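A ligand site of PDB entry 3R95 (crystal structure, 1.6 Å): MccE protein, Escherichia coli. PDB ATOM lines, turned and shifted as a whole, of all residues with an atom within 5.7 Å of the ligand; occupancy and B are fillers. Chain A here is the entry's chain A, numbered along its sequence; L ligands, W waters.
N of Lys 118 is in hydrogen-bond range of O6 of the ligand (3.3 Å).
N of Val 121 is in hydrogen-bond range of O9 of the ligand.
An oxygen (O14) of the ligand lies within hydrogen-bond range of the side-chain amide oxygen (OE1) of Gln 116, at 3.4 Å.
The backbone carbonyl oxygen (O) of Tyr 109 lies within hydrogen-bond range of a nitrogen (N7) of the ligand.
ND2 of Asn 149 is in hydrogen-bond range of O16 of the ligand.
The side-chain hydroxyl of Thr 122 lies within hydrogen-bond range of an oxygen (O8) of the ligand (2.8 Å).
The backbone NH (N) of Tyr 109 lies within hydrogen-bond range of an oxygen (O17) of the ligand (3.1 Å).
O8 of the ligand lies within hydrogen-bond range of OG1 of Thr 155 (3.0 Å).
An oxygen (O6) of the ligand sits at hydrogen-bond distance from the backbone NH of Gly 119 (3.1 Å).
OG of Ser 152 sits close to S1 of the ligand, 3.3 Å away.
O15 of the ligand lies within hydrogen-bond range of N of Leu 111 (2.8 Å).
An oxygen (O8) of the ligand is in salt-bridge range of the guanidinium group of Arg 158, at 2.8 Å.
The backbone NH (N) of Thr 122 is in hydrogen-bond range of an oxygen (O9) of the ligand (2.8 Å).
The backbone NH (N) of Ile 120 sits at hydrogen-bond distance from an oxygen (O9) of the ligand (3.2 Å).
OG of Ser 49 lies close to O16 of the ligand, 3.4 Å away.
The backbone NH of Gly 117 is in hydrogen-bond range of an oxygen (O11) of the ligand (2.8 Å).
The side-chain hydroxyl (OG) of Ser 49 lies within hydrogen-bond range of the backbone carbonyl oxygen (O) of Phe 46, 3.4 Å away.
The backbone NH (N) of Ser 152 sits at hydrogen-bond distance from the side-chain amide oxygen (OD1) of Asn 149 (3.1 Å).
The side-chain amide nitrogen (ND2) of Asn 123 lies within hydrogen-bond range of the backbone carbonyl oxygen (O) of Gly 119.
O of Leu 111 sits at hydrogen-bond distance from NE2 of Gln 116, at 3.0 Å.
OH of Tyr 109 lies within hydrogen-bond range of OG of Ser 152, at 3.0 Å.
The side-chain hydroxyl (OG1) of Thr 155 is in hydrogen-bond range of the backbone carbonyl oxygen (O) of Lys 151 (3.1 Å).
The side-chain hydroxyl (OG) of Ser 152 sits close to the side-chain sulfur (SG) of Cys 145 (3.8 Å).
Merely in contact with the ligand: Met 50, Ile 107, Gly 108, Trp 110, Ile 143, Lys 144, Cys 145 and Lys 151.
Hydrophobic or aromatic side chains within 4 Å of the ligand: Met 50, Tyr 109, Trp 110, Leu 111, Val 121 and Ile 143.
Of the 30 residues printed, 22 come within 4 Å of the ligand.
Water W1 lies within hydrogen-bond range of an oxygen (O12) of the ligand, the backbone carbonyl oxygen of Lys 151, the guanidinium group of Arg 158 and the side-chain hydroxyl of Thr 155.
Water W9 lies within hydrogen-bond range of an oxygen (O12) of the ligand (2.7 Å) and the backbone NH (N) of Gly 117 (3.5 Å).
Water W7 bridges an oxygen (O4) of the ligand (2.7 Å) and the guanidinium group (NH2) of Arg 158 (3.0 Å).
Water W5 bridges O5 of the ligand (2.8 Å) and NH2 of Arg 158 (3.1 Å).
Water W6 lies within hydrogen-bond range of the side-chain amide nitrogen of Asn 123 (2.8 Å) and a nitrogen (N3) of the ligand (3.4 Å).
Water W2 bridges the backbone carbonyl oxygen (O) of Asn 45 and the side-chain hydroxyl (OG) of Ser 49.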
ATOM      1  N   ASN A  45     -13.704  11.218  -5.025  1.00  0.00           N
ATOM      2  CA  ASN A  45     -13.160  11.478  -3.690  1.00  0.00           C
ATOM      3  C   ASN A  45     -13.490  10.385  -2.674  1.00  0.00           C
ATOM      4  O   ASN A  45     -12.656  10.050  -1.835  1.00  0.00           O
ATOM      5  CB  ASN A  45     -13.512  12.886  -3.165  1.00  0.00           C
ATOM      6  CG  ASN A  45     -14.974  13.263  -3.374  1.00  0.00           C
ATOM      7  OD1 ASN A  45     -15.433  13.398  -4.511  1.00  0.00           O
ATOM      8  ND2 ASN A  45     -15.699  13.468  -2.280  1.00  0.00           N
ATOM      9  N   PHE A  46     -14.704   9.823  -2.757  1.00  0.00           N
ATOM     10  CA  PHE A  46     -15.153   8.779  -1.831  1.00  0.00           C
ATOM     11  C   PHE A  46     -14.397   7.452  -1.965  1.00  0.00           C
ATOM     12  O   PHE A  46     -14.206   6.744  -0.979  1.00  0.00           O
ATOM     13  CB  PHE A  46     -16.662   8.510  -1.999  1.00  0.00           C
ATOM     14  CG  PHE A  46     -17.548   9.506  -1.298  1.00  0.00           C
ATOM     15  CD1 PHE A  46     -17.018  10.529  -0.505  1.00  0.00           C
ATOM     16  CD2 PHE A  46     -18.925   9.408  -1.418  1.00  0.00           C
ATOM     17  CE1 PHE A  46     -17.845  11.431   0.133  1.00  0.00           C
ATOM     18  CE2 PHE A  46     -19.765  10.304  -0.768  1.00  0.00           C
ATOM     19  CZ  PHE A  46     -19.222  11.319   0.008  1.00  0.00           C
ATOM     20  N   SER A  49     -11.451   6.603   0.350  1.00  0.00           N
ATOM     21  CA  SER A  49     -11.661   6.316   1.778  1.00  0.00           C
ATOM     22  C   SER A  49     -12.637   5.183   2.090  1.00  0.00           C
ATOM     23  O   SER A  49     -12.658   4.689   3.217  1.00  0.00           O
ATOM     24  CB  SER A  49     -12.098   7.581   2.511  1.00  0.00           C
ATOM     25  OG  SER A  49     -13.322   8.070   1.986  1.00  0.00           O
ATOM     26  N   MET A  50     -13.469   4.803   1.121  1.00  0.00           N
ATOM     27  CA  MET A  50     -14.529   3.809   1.353  1.00  0.00           C
ATOM     28  C   MET A  50     -14.614   2.799   0.208  1.00  0.00           C
ATOM     29  O   MET A  50     -14.251   3.105  -0.930  1.00  0.00           O
ATOM     30  CB  MET A  50     -15.882   4.504   1.559  1.00  0.00           C
ATOM     31  CG  MET A  50     -15.928   5.435   2.783  1.00  0.00           C
ATOM     32  SD  MET A  50     -17.474   6.333   2.945  1.00  0.00           S
ATOM     33  CE  MET A  50     -17.464   7.330   1.461  1.00  0.00           C
ATOM     34  N   ASN A  96     -23.605   1.019  11.994  1.00  0.00           N
ATOM     35  CA  ASN A  96     -23.466  -0.004  10.956  1.00  0.00           C
ATOM     36  C   ASN A  96     -23.743  -1.399  11.502  1.00  0.00           C
ATOM     37  O   ASN A  96     -24.272  -2.263  10.788  1.00  0.00           O
ATOM     38  CB  ASN A  96     -22.070   0.044  10.344  1.00  0.00           C
ATOM     39  CG  ASN A  96     -21.889   1.193   9.380  1.00  0.00           C
ATOM     40  OD1 ASN A  96     -22.856   1.650   8.761  1.00  0.00           O
ATOM     41  ND2 ASN A  96     -20.662   1.654   9.219  1.00  0.00           N
ATOM     42  N   ILE A 107     -20.131   2.776  14.766  1.00  0.00           N
ATOM     43  CA  ILE A 107     -20.561   3.981  14.048  1.00  0.00           C
ATOM     44  C   ILE A 107     -19.876   4.144  12.690  1.00  0.00           C
ATOM     45  O   ILE A 107     -18.682   3.881  12.555  1.00  0.00           O
ATOM     46  CB  ILE A 107     -20.327   5.245  14.911  1.00  0.00           C
ATOM     47  CG1 ILE A 107     -21.280   5.241  16.122  1.00  0.00           C
ATOM     48  CG2 ILE A 107     -20.473   6.523  14.073  1.00  0.00           C
ATOM     49  CD1 ILE A 107     -20.917   6.250  17.194  1.00  0.00           C
ATOM     50  N   GLY A 108     -20.648   4.570  11.702  1.00  0.00           N
ATOM     51  CA  GLY A 108     -20.107   4.937  10.391  1.00  0.00           C
ATOM     52  C   GLY A 108     -20.635   6.295   9.967  1.00  0.00           C
ATOM     53  O   GLY A 108     -21.694   6.734  10.438  1.00  0.00           O
ATOM     54  N   TYR A 109     -19.911   6.963   9.082  1.00  0.00           N
ATOM     55  CA  TYR A 109     -20.330   8.271   8.572  1.00  0.00           C
ATOM     56  C   TYR A 109     -19.662   8.657   7.268  1.00  0.00           C
ATOM     57  O   TYR A 109     -18.530   8.276   7.007  1.00  0.00           O
ATOM     58  CB  TYR A 109     -20.083   9.378   9.619  1.00  0.00           C
ATOM     59  CG  TYR A 109     -18.769   9.274  10.370  1.00  0.00           C
ATOM     60  CD1 TYR A 109     -17.585   9.777   9.826  1.00  0.00           C
ATOM     61  CD2 TYR A 109     -18.719   8.706  11.640  1.00  0.00           C
ATOM     62  CE1 TYR A 109     -16.380   9.690  10.527  1.00  0.00           C
ATOM     63  CE2 TYR A 109     -17.534   8.619  12.355  1.00  0.00           C
ATOM     64  CZ  TYR A 109     -16.365   9.111  11.799  1.00  0.00           C
ATOM     65  OH  TYR A 109     -15.186   9.017  12.512  1.00  0.00           O
ATOM     66  N   TRP A 110     -20.387   9.423   6.461  1.00  0.00           N
ATOM     67  CA  TRP A 110     -19.794  10.125   5.328  1.00  0.00           C
ATOM     68  C   TRP A 110     -20.609  11.346   4.954  1.00  0.00           C
ATOM     69  O   TRP A 110     -21.817  11.389   5.184  1.00  0.00           O
ATOM     70  CB  TRP A 110     -19.569   9.208   4.111  1.00  0.00           C
ATOM     71  CG  TRP A 110     -20.780   8.487   3.561  1.00  0.00           C
ATOM     72  CD1 TRP A 110     -21.166   7.210   3.825  1.00  0.00           C
ATOM     73  CD2 TRP A 110     -21.716   9.003   2.598  1.00  0.00           C
ATOM     74  NE1 TRP A 110     -22.293   6.895   3.114  1.00  0.00           N
ATOM     75  CE2 TRP A 110     -22.651   7.976   2.352  1.00  0.00           C
ATOM     76  CE3 TRP A 110     -21.865  10.223   1.946  1.00  0.00           C
ATOM     77  CZ2 TRP A 110     -23.718   8.138   1.460  1.00  0.00           C
ATOM     78  CZ3 TRP A 110     -22.926  10.392   1.055  1.00  0.00           C
ATOM     79  CH2 TRP A 110     -23.849   9.349   0.833  1.00  0.00           C
ATOM     80  N   LEU A 111     -19.934  12.339   4.383  1.00  0.00           N
ATOM     81  CA  LEU A 111     -20.561  13.575   3.925  1.00  0.00           C
ATOM     82  C   LEU A 111     -20.066  13.933   2.542  1.00  0.00           C
ATOM     83  O   LEU A 111     -18.891  13.750   2.224  1.00  0.00           O
ATOM     84  CB  LEU A 111     -20.202  14.741   4.833  1.00  0.00           C
ATOM     85  CG  LEU A 111     -20.818  14.837   6.223  1.00  0.00           C
ATOM     86  CD1 LEU A 111     -20.112  15.962   6.961  1.00  0.00           C
ATOM     87  CD2 LEU A 111     -22.315  15.081   6.174  1.00  0.00           C
ATOM     88  N   GLY A 112     -20.962  14.485   1.730  1.00  0.00           N
ATOM     89  CA  GLY A 112     -20.565  15.097   0.462  1.00  0.00           C
ATOM     90  C   GLY A 112     -19.588  16.221   0.719  1.00  0.00           C
ATOM     91  O   GLY A 112     -19.646  16.892   1.757  1.00  0.00           O
ATOM     92  N   PHE A 115     -20.573  19.597   2.094  1.00  0.00           N
ATOM     93  CA  PHE A 115     -21.129  19.609   3.437  1.00  0.00           C
ATOM     94  C   PHE A 115     -20.087  19.394   4.521  1.00  0.00           C
ATOM     95  O   PHE A 115     -20.405  19.407   5.711  1.00  0.00           O
ATOM     96  CB  PHE A 115     -22.241  18.568   3.560  1.00  0.00           C
ATOM     97  CG  PHE A 115     -23.341  18.762   2.555  1.00  0.00           C
ATOM     98  CD1 PHE A 115     -24.374  19.664   2.801  1.00  0.00           C
ATOM     99  CD2 PHE A 115     -23.344  18.050   1.357  1.00  0.00           C
ATOM    100  CE1 PHE A 115     -25.392  19.860   1.870  1.00  0.00           C
ATOM    101  CE2 PHE A 115     -24.353  18.224   0.426  1.00  0.00           C
ATOM    102  CZ  PHE A 115     -25.386  19.139   0.677  1.00  0.00           C
ATOM    103  N   GLN A 116     -18.838  19.207   4.112  1.00  0.00           N
ATOM    104  CA  GLN A 116     -17.740  19.017   5.053  1.00  0.00           C
ATOM    105  C   GLN A 116     -17.263  20.359   5.606  1.00  0.00           C
ATOM    106  O   GLN A 116     -17.443  21.398   4.959  1.00  0.00           O
ATOM    107  CB  GLN A 116     -16.586  18.250   4.390  1.00  0.00           C
ATOM    108  CG  GLN A 116     -16.936  16.794   4.095  1.00  0.00           C
ATOM    109  CD  GLN A 116     -15.854  16.046   3.344  1.00  0.00           C
ATOM    110  OE1 GLN A 116     -14.670  16.382   3.446  1.00  0.00           O
ATOM    111  NE2 GLN A 116     -16.250  15.027   2.594  1.00  0.00           N
ATOM    112  N   GLY A 117     -16.707  20.339   6.808  1.00  0.00           N
ATOM    113  CA  GLY A 117     -16.191  21.553   7.443  1.00  0.00           C
ATOM    114  C   GLY A 117     -17.262  22.355   8.161  1.00  0.00           C
ATOM    115  O   GLY A 117     -17.053  23.538   8.463  1.00  0.00           O
ATOM    116  N   LYS A 118     -18.386  21.709   8.455  1.00  0.00           N
ATOM    117  CA  LYS A 118     -19.536  22.373   9.073  1.00  0.00           C
ATOM    118  C   LYS A 118     -19.953  21.761  10.410  1.00  0.00           C
ATOM    119  O   LYS A 118     -20.956  22.172  11.003  1.00  0.00           O
ATOM    120  CB  LYS A 118     -20.736  22.369   8.123  1.00  0.00           C
ATOM    121  CG  LYS A 118     -20.561  23.209   6.873  1.00  0.00           C
ATOM    122  CD  LYS A 118     -21.744  22.990   5.938  1.00  0.00           C
ATOM    123  CE  LYS A 118     -21.765  24.008   4.811  1.00  0.00           C
ATOM    124  NZ  LYS A 118     -22.175  25.356   5.287  1.00  0.00           N
ATOM    125  N   GLY A 119     -19.192  20.771  10.883  1.00  0.00           N
ATOM    126  CA  GLY A 119     -19.519  20.083  12.138  1.00  0.00           C
ATOM    127  C   GLY A 119     -20.756  19.209  12.113  1.00  0.00           C
ATOM    128  O   GLY A 119     -21.288  18.832  13.164  1.00  0.00           O
ATOM    129  N   ILE A 120     -21.200  18.864  10.911  1.00  0.00           N
ATOM    130  CA  ILE A 120     -22.437  18.113  10.728  1.00  0.00           C
ATOM    131  C   ILE A 120     -22.393  16.719  11.359  1.00  0.00           C
ATOM    132  O   ILE A 120     -23.339  16.319  12.046  1.00  0.00           O
ATOM    133  CB  ILE A 120     -22.821  18.025   9.228  1.00  0.00           C
ATOM    134  CG1 ILE A 120     -23.047  19.425   8.633  1.00  0.00           C
ATOM    135  CG2 ILE A 120     -24.060  17.130   9.018  1.00  0.00           C
ATOM    136  CD1 ILE A 120     -24.021  20.259   9.358  1.00  0.00           C
ATOM    137  N   VAL A 121     -21.314  15.983  11.110  1.00  0.00           N
ATOM    138  CA  VAL A 121     -21.189  14.613  11.625  1.00  0.00           C
ATOM    139  C   VAL A 121     -20.951  14.612  13.136  1.00  0.00           C
ATOM    140  O   VAL A 121     -21.548  13.801  13.848  1.00  0.00           O
ATOM    141  CB  VAL A 121     -20.123  13.801  10.860  1.00  0.00           C
ATOM    142  CG1 VAL A 121     -19.700  12.556  11.650  1.00  0.00           C
ATOM    143  CG2 VAL A 121     -20.674  13.395   9.518  1.00  0.00           C
ATOM    144  N   THR A 122     -20.122  15.523  13.617  1.00  0.00           N
ATOM    145  CA  THR A 122     -19.902  15.679  15.067  1.00  0.00           C
ATOM    146  C   THR A 122     -21.218  15.956  15.792  1.00  0.00           C
ATOM    147  O   THR A 122     -21.527  15.307  16.785  1.00  0.00           O
ATOM    148  CB  THR A 122     -18.852  16.767  15.361  1.00  0.00           C
ATOM    149  OG1 THR A 122     -17.567  16.276  14.980  1.00  0.00           O
ATOM    150  CG2 THR A 122     -18.820  17.114  16.850  1.00  0.00           C
ATOM    151  N   ASN A 123     -22.002  16.910  15.275  1.00  0.00           N
ATOM    152  CA  ASN A 123     -23.309  17.189  15.856  1.00  0.00           C
ATOM    153  C   ASN A 123     -24.248  15.989  15.813  1.00  0.00           C
ATOM    154  O   ASN A 123     -24.952  15.709  16.783  1.00  0.00           O
ATOM    155  CB  ASN A 123     -23.970  18.401  15.184  1.00  0.00           C
ATOM    156  CG  ASN A 123     -23.432  19.725  15.696  1.00  0.00           C
ATOM    157  OD1 ASN A 123     -23.207  19.901  16.889  1.00  0.00           O
ATOM    158  ND2 ASN A 123     -23.280  20.678  14.786  1.00  0.00           N
ATOM    159  N   ILE A 143     -15.910   3.674  17.076  1.00  0.00           N
ATOM    160  CA  ILE A 143     -15.529   4.151  15.742  1.00  0.00           C
ATOM    161  C   ILE A 143     -14.235   3.469  15.322  1.00  0.00           C
ATOM    162  O   ILE A 143     -13.224   3.562  16.014  1.00  0.00           O
ATOM    163  CB  ILE A 143     -15.367   5.693  15.678  1.00  0.00           C
ATOM    164  CG1 ILE A 143     -16.717   6.394  15.907  1.00  0.00           C
ATOM    165  CG2 ILE A 143     -14.795   6.123  14.333  1.00  0.00           C
ATOM    166  CD1 ILE A 143     -16.601   7.897  16.210  1.00  0.00           C
ATOM    167  N   LYS A 144     -14.287   2.771  14.194  1.00  0.00           N
ATOM    168  CA  LYS A 144     -13.096   2.191  13.582  1.00  0.00           C
ATOM    169  C   LYS A 144     -12.817   2.957  12.303  1.00  0.00           C
ATOM    170  O   LYS A 144     -13.717   3.126  11.482  1.00  0.00           O
ATOM    171  CB  LYS A 144     -13.324   0.721  13.226  1.00  0.00           C
ATOM    172  CG  LYS A 144     -13.477  -0.229  14.392  1.00  0.00           C
ATOM    173  CD  LYS A 144     -13.817  -1.596  13.825  1.00  0.00           C
ATOM    174  CE  LYS A 144     -13.765  -2.696  14.845  1.00  0.00           C
ATOM    175  NZ  LYS A 144     -14.166  -3.967  14.175  1.00  0.00           N
ATOM    176  N   CYS A 145     -11.581   3.399  12.132  1.00  0.00           N
ATOM    177  CA  CYS A 145     -11.217   4.089  10.893  1.00  0.00           C
ATOM    178  C   CYS A 145      -9.742   3.908  10.566  1.00  0.00           C
ATOM    179  O   CYS A 145      -8.900   3.829  11.458  1.00  0.00           O
ATOM    180  CB  CYS A 145     -11.575   5.577  10.968  1.00  0.00           C
ATOM    181  SG  CYS A 145     -10.748   6.499  12.270  1.00  0.00           S
ATOM    182  N   ILE A 146      -9.457   3.870   9.272  1.00  0.00           N
ATOM    183  CA  ILE A 146      -8.095   3.679   8.796  1.00  0.00           C
ATOM    184  C   ILE A 146      -7.162   4.748   9.369  1.00  0.00           C
ATOM    185  O   ILE A 146      -7.534   5.923   9.467  1.00  0.00           O
ATOM    186  CB  ILE A 146      -8.057   3.602   7.244  1.00  0.00           C
ATOM    187  CG1 ILE A 146      -8.698   2.292   6.779  1.00  0.00           C
ATOM    188  CG2 ILE A 146      -6.636   3.717   6.712  1.00  0.00           C
ATOM    189  CD1 ILE A 146      -9.032   2.234   5.304  1.00  0.00           C
ATOM    190  N   ASN A 149      -6.647   8.070   7.586  1.00  0.00           N
ATOM    191  CA  ASN A 149      -7.830   8.899   7.310  1.00  0.00           C
ATOM    192  C   ASN A 149      -7.886  10.069   8.285  1.00  0.00           C
ATOM    193  O   ASN A 149      -8.457   9.968   9.373  1.00  0.00           O
ATOM    194  CB  ASN A 149      -9.112   8.062   7.353  1.00  0.00           C
ATOM    195  CG  ASN A 149     -10.335   8.813   6.829  1.00  0.00           C
ATOM    196  OD1 ASN A 149     -10.432  10.038   6.931  1.00  0.00           O
ATOM    197  ND2 ASN A 149     -11.298   8.068   6.291  1.00  0.00           N
ATOM    198  N   LYS A 151      -9.388  13.120   8.423  1.00  0.00           N
ATOM    199  CA  LYS A 151     -10.660  13.718   8.826  1.00  0.00           C
ATOM    200  C   LYS A 151     -11.511  12.797   9.691  1.00  0.00           C
ATOM    201  O   LYS A 151     -12.179  13.256  10.618  1.00  0.00           O
ATOM    202  CB  LYS A 151     -11.441  14.189   7.594  1.00  0.00           C
ATOM    203  CG  LYS A 151     -10.858  15.444   6.976  1.00  0.00           C
ATOM    204  CD  LYS A 151     -11.572  15.838   5.698  1.00  0.00           C
ATOM    205  CE  LYS A 151     -11.501  17.353   5.474  1.00  0.00           C
ATOM    206  NZ  LYS A 151     -10.156  17.928   5.737  1.00  0.00           N
ATOM    207  N   SER A 152     -11.503  11.493   9.407  1.00  0.00           N
ATOM    208  CA  SER A 152     -12.290  10.569  10.215  1.00  0.00           C
ATOM    209  C   SER A 152     -11.741  10.431  11.633  1.00  0.00           C
ATOM    210  O   SER A 152     -12.509  10.390  12.596  1.00  0.00           O
ATOM    211  CB  SER A 152     -12.411   9.189   9.558  1.00  0.00           C
ATOM    212  OG  SER A 152     -13.328   8.389  10.300  1.00  0.00           O
ATOM    213  N   ALA A 154     -10.003  12.746  13.187  1.00  0.00           N
ATOM    214  CA  ALA A 154     -10.313  14.031  13.818  1.00  0.00           C
ATOM    215  C   ALA A 154     -11.743  14.072  14.364  1.00  0.00           C
ATOM    216  O   ALA A 154     -11.983  14.577  15.463  1.00  0.00           O
ATOM    217  CB  ALA A 154     -10.061  15.171  12.847  1.00  0.00           C
ATOM    218  N   THR A 155     -12.689  13.538  13.592  1.00  0.00           N
ATOM    219  CA  THR A 155     -14.091  13.478  14.001  1.00  0.00           C
ATOM    220  C   THR A 155     -14.269  12.623  15.267  1.00  0.00           C
ATOM    221  O   THR A 155     -14.959  13.032  16.199  1.00  0.00           O
ATOM    222  CB  THR A 155     -14.985  12.968  12.844  1.00  0.00           C
ATOM    223  OG1 THR A 155     -14.955  13.922  11.779  1.00  0.00           O
ATOM    224  CG2 THR A 155     -16.436  12.762  13.299  1.00  0.00           C
ATOM    225  N   ARG A 158     -12.969  14.582  18.152  1.00  0.00           N
ATOM    226  CA  ARG A 158     -13.863  15.730  18.345  1.00  0.00           C
ATOM    227  C   ARG A 158     -15.122  15.347  19.119  1.00  0.00           C
ATOM    228  O   ARG A 158     -15.675  16.164  19.858  1.00  0.00           O
ATOM    229  CB  ARG A 158     -14.232  16.329  16.970  1.00  0.00           C
ATOM    230  CG  ARG A 158     -14.899  17.696  17.006  1.00  0.00           C
ATOM    231  CD  ARG A 158     -15.013  18.288  15.603  1.00  0.00           C
ATOM    232  NE  ARG A 158     -13.716  18.652  15.035  1.00  0.00           N
ATOM    233  CZ  ARG A 158     -13.113  18.025  14.026  1.00  0.00           C
ATOM    234  NH1 ARG A 158     -13.672  16.978  13.426  1.00  0.00           N
ATOM    235  NH2 ARG A 158     -11.927  18.455  13.594  1.00  0.00           N
HETATM  236  N1  LIG L   1     -19.027  21.947  15.384  1.00  0.00           N
HETATM  237  C1  LIG L   1     -17.906  21.238  15.150  1.00  0.00           C
HETATM  238  N2  LIG L   1     -17.127  21.489  14.076  1.00  0.00           N
HETATM  239  C2  LIG L   1     -17.447  22.491  13.218  1.00  0.00           C
HETATM  240  C3  LIG L   1     -18.595  23.242  13.443  1.00  0.00           C
HETATM  241  C4  LIG L   1     -19.388  22.953  14.547  1.00  0.00           C
HETATM  242  N3  LIG L   1     -20.504  23.673  14.774  1.00  0.00           N
HETATM  243  N4  LIG L   1     -18.707  24.152  12.463  1.00  0.00           N
HETATM  244  C5  LIG L   1     -17.646  23.981  11.643  1.00  0.00           C
HETATM  245  N5  LIG L   1     -16.878  22.986  12.112  1.00  0.00           N
HETATM  246  C6  LIG L   1     -15.661  22.507  11.396  1.00  0.00           C
HETATM  247  C7  LIG L   1     -14.433  22.101  12.176  1.00  0.00           C
HETATM  248  O1  LIG L   1     -13.511  23.181  12.314  1.00  0.00           O
HETATM  249  C8  LIG L   1     -13.856  20.985  11.326  1.00  0.00           C
HETATM  250  O2  LIG L   1     -13.222  21.545  10.169  1.00  0.00           O
HETATM  251  P1  LIG L   1     -11.676  21.289   9.775  1.00  0.00           P
HETATM  252  O3  LIG L   1     -11.411  22.342   8.720  1.00  0.00           O
HETATM  253  O4  LIG L   1     -11.634  19.879   9.240  1.00  0.00           O
HETATM  254  O5  LIG L   1     -10.916  21.486  11.065  1.00  0.00           O
HETATM  255  C9  LIG L   1     -15.087  20.278  10.798  1.00  0.00           C
HETATM  256  O6  LIG L   1     -16.098  21.287  10.765  1.00  0.00           O
HETATM  257  C10 LIG L   1     -15.523  19.111  11.669  1.00  0.00           C
HETATM  258  O7  LIG L   1     -16.777  18.619  11.193  1.00  0.00           O
HETATM  259  P2  LIG L   1     -17.249  17.097  11.477  1.00  0.00           P
HETATM  260  O8  LIG L   1     -16.324  16.491  12.504  1.00  0.00           O
HETATM  261  O9  LIG L   1     -18.724  17.038  11.768  1.00  0.00           O
HETATM  262  O10 LIG L   1     -17.006  16.319  10.084  1.00  0.00           O
HETATM  263  P3  LIG L   1     -16.231  16.808   8.749  1.00  0.00           P
HETATM  264  O11 LIG L   1     -17.062  17.860   8.073  1.00  0.00           O
HETATM  265  O12 LIG L   1     -14.800  17.148   9.083  1.00  0.00           O
HETATM  266  O13 LIG L   1     -16.315  15.466   7.870  1.00  0.00           O
HETATM  267  C11 LIG L   1     -15.913  13.117   7.385  1.00  0.00           C
HETATM  268  C12 LIG L   1     -15.569  14.317   8.266  1.00  0.00           C
HETATM  269  C13 LIG L   1     -15.011  11.954   7.812  1.00  0.00           C
HETATM  270  C14 LIG L   1     -17.375  12.764   7.647  1.00  0.00           C
HETATM  271  C15 LIG L   1     -15.661  13.498   5.924  1.00  0.00           C
HETATM  272  O14 LIG L   1     -14.304  13.952   5.758  1.00  0.00           O
HETATM  273  C16 LIG L   1     -15.978  12.419   4.913  1.00  0.00           C
HETATM  274  O15 LIG L   1     -17.138  12.140   4.665  1.00  0.00           O
HETATM  275  N6  LIG L   1     -14.953  11.808   4.319  1.00  0.00           N
HETATM  276  C17 LIG L   1     -14.981  10.754   3.298  1.00  0.00           C
HETATM  277  C18 LIG L   1     -15.650   9.494   3.864  1.00  0.00           C
HETATM  278  C19 LIG L   1     -14.950   8.997   5.111  1.00  0.00           C
HETATM  279  O16 LIG L   1     -13.736   9.045   5.205  1.00  0.00           O
HETATM  280  N7  LIG L   1     -15.733   8.524   6.090  1.00  0.00           N
HETATM  281  C20 LIG L   1     -15.291   8.006   7.375  1.00  0.00           C
HETATM  282  C21 LIG L   1     -15.095   6.500   7.202  1.00  0.00           C
HETATM  283  S1  LIG L   1     -14.564   5.808   8.738  1.00  0.00           S
HETATM  284  C22 LIG L   1     -16.033   5.668   9.534  1.00  0.00           C
HETATM  285  O17 LIG L   1     -17.096   5.685   8.920  1.00  0.00           O
HETATM  286  C23 LIG L   1     -16.033   5.518  11.025  1.00  0.00           C
HETATM  287  O   HOH W   1     -12.934  16.102  10.653  1.00  0.00           O
HETATM  288  O   HOH W   2     -12.726  10.415   0.751  1.00  0.00           O
HETATM  289  O   HOH W   3     -13.077  24.802  10.225  1.00  0.00           O
HETATM  290  O   HOH W   4     -19.527  19.024   8.342  1.00  0.00           O
HETATM  291  O   HOH W   5     -11.466  21.517  13.762  1.00  0.00           O
HETATM  292  O   HOH W   6     -23.855  23.401  15.088  1.00  0.00           O
HETATM  293  O   HOH W   7     -10.923  17.754  10.803  1.00  0.00           O
HETATM  294  O   HOH W   8     -11.923  11.308   4.925  1.00  0.00           O
HETATM  295  O   HOH W   9     -13.602  18.999   7.559  1.00  0.00           O
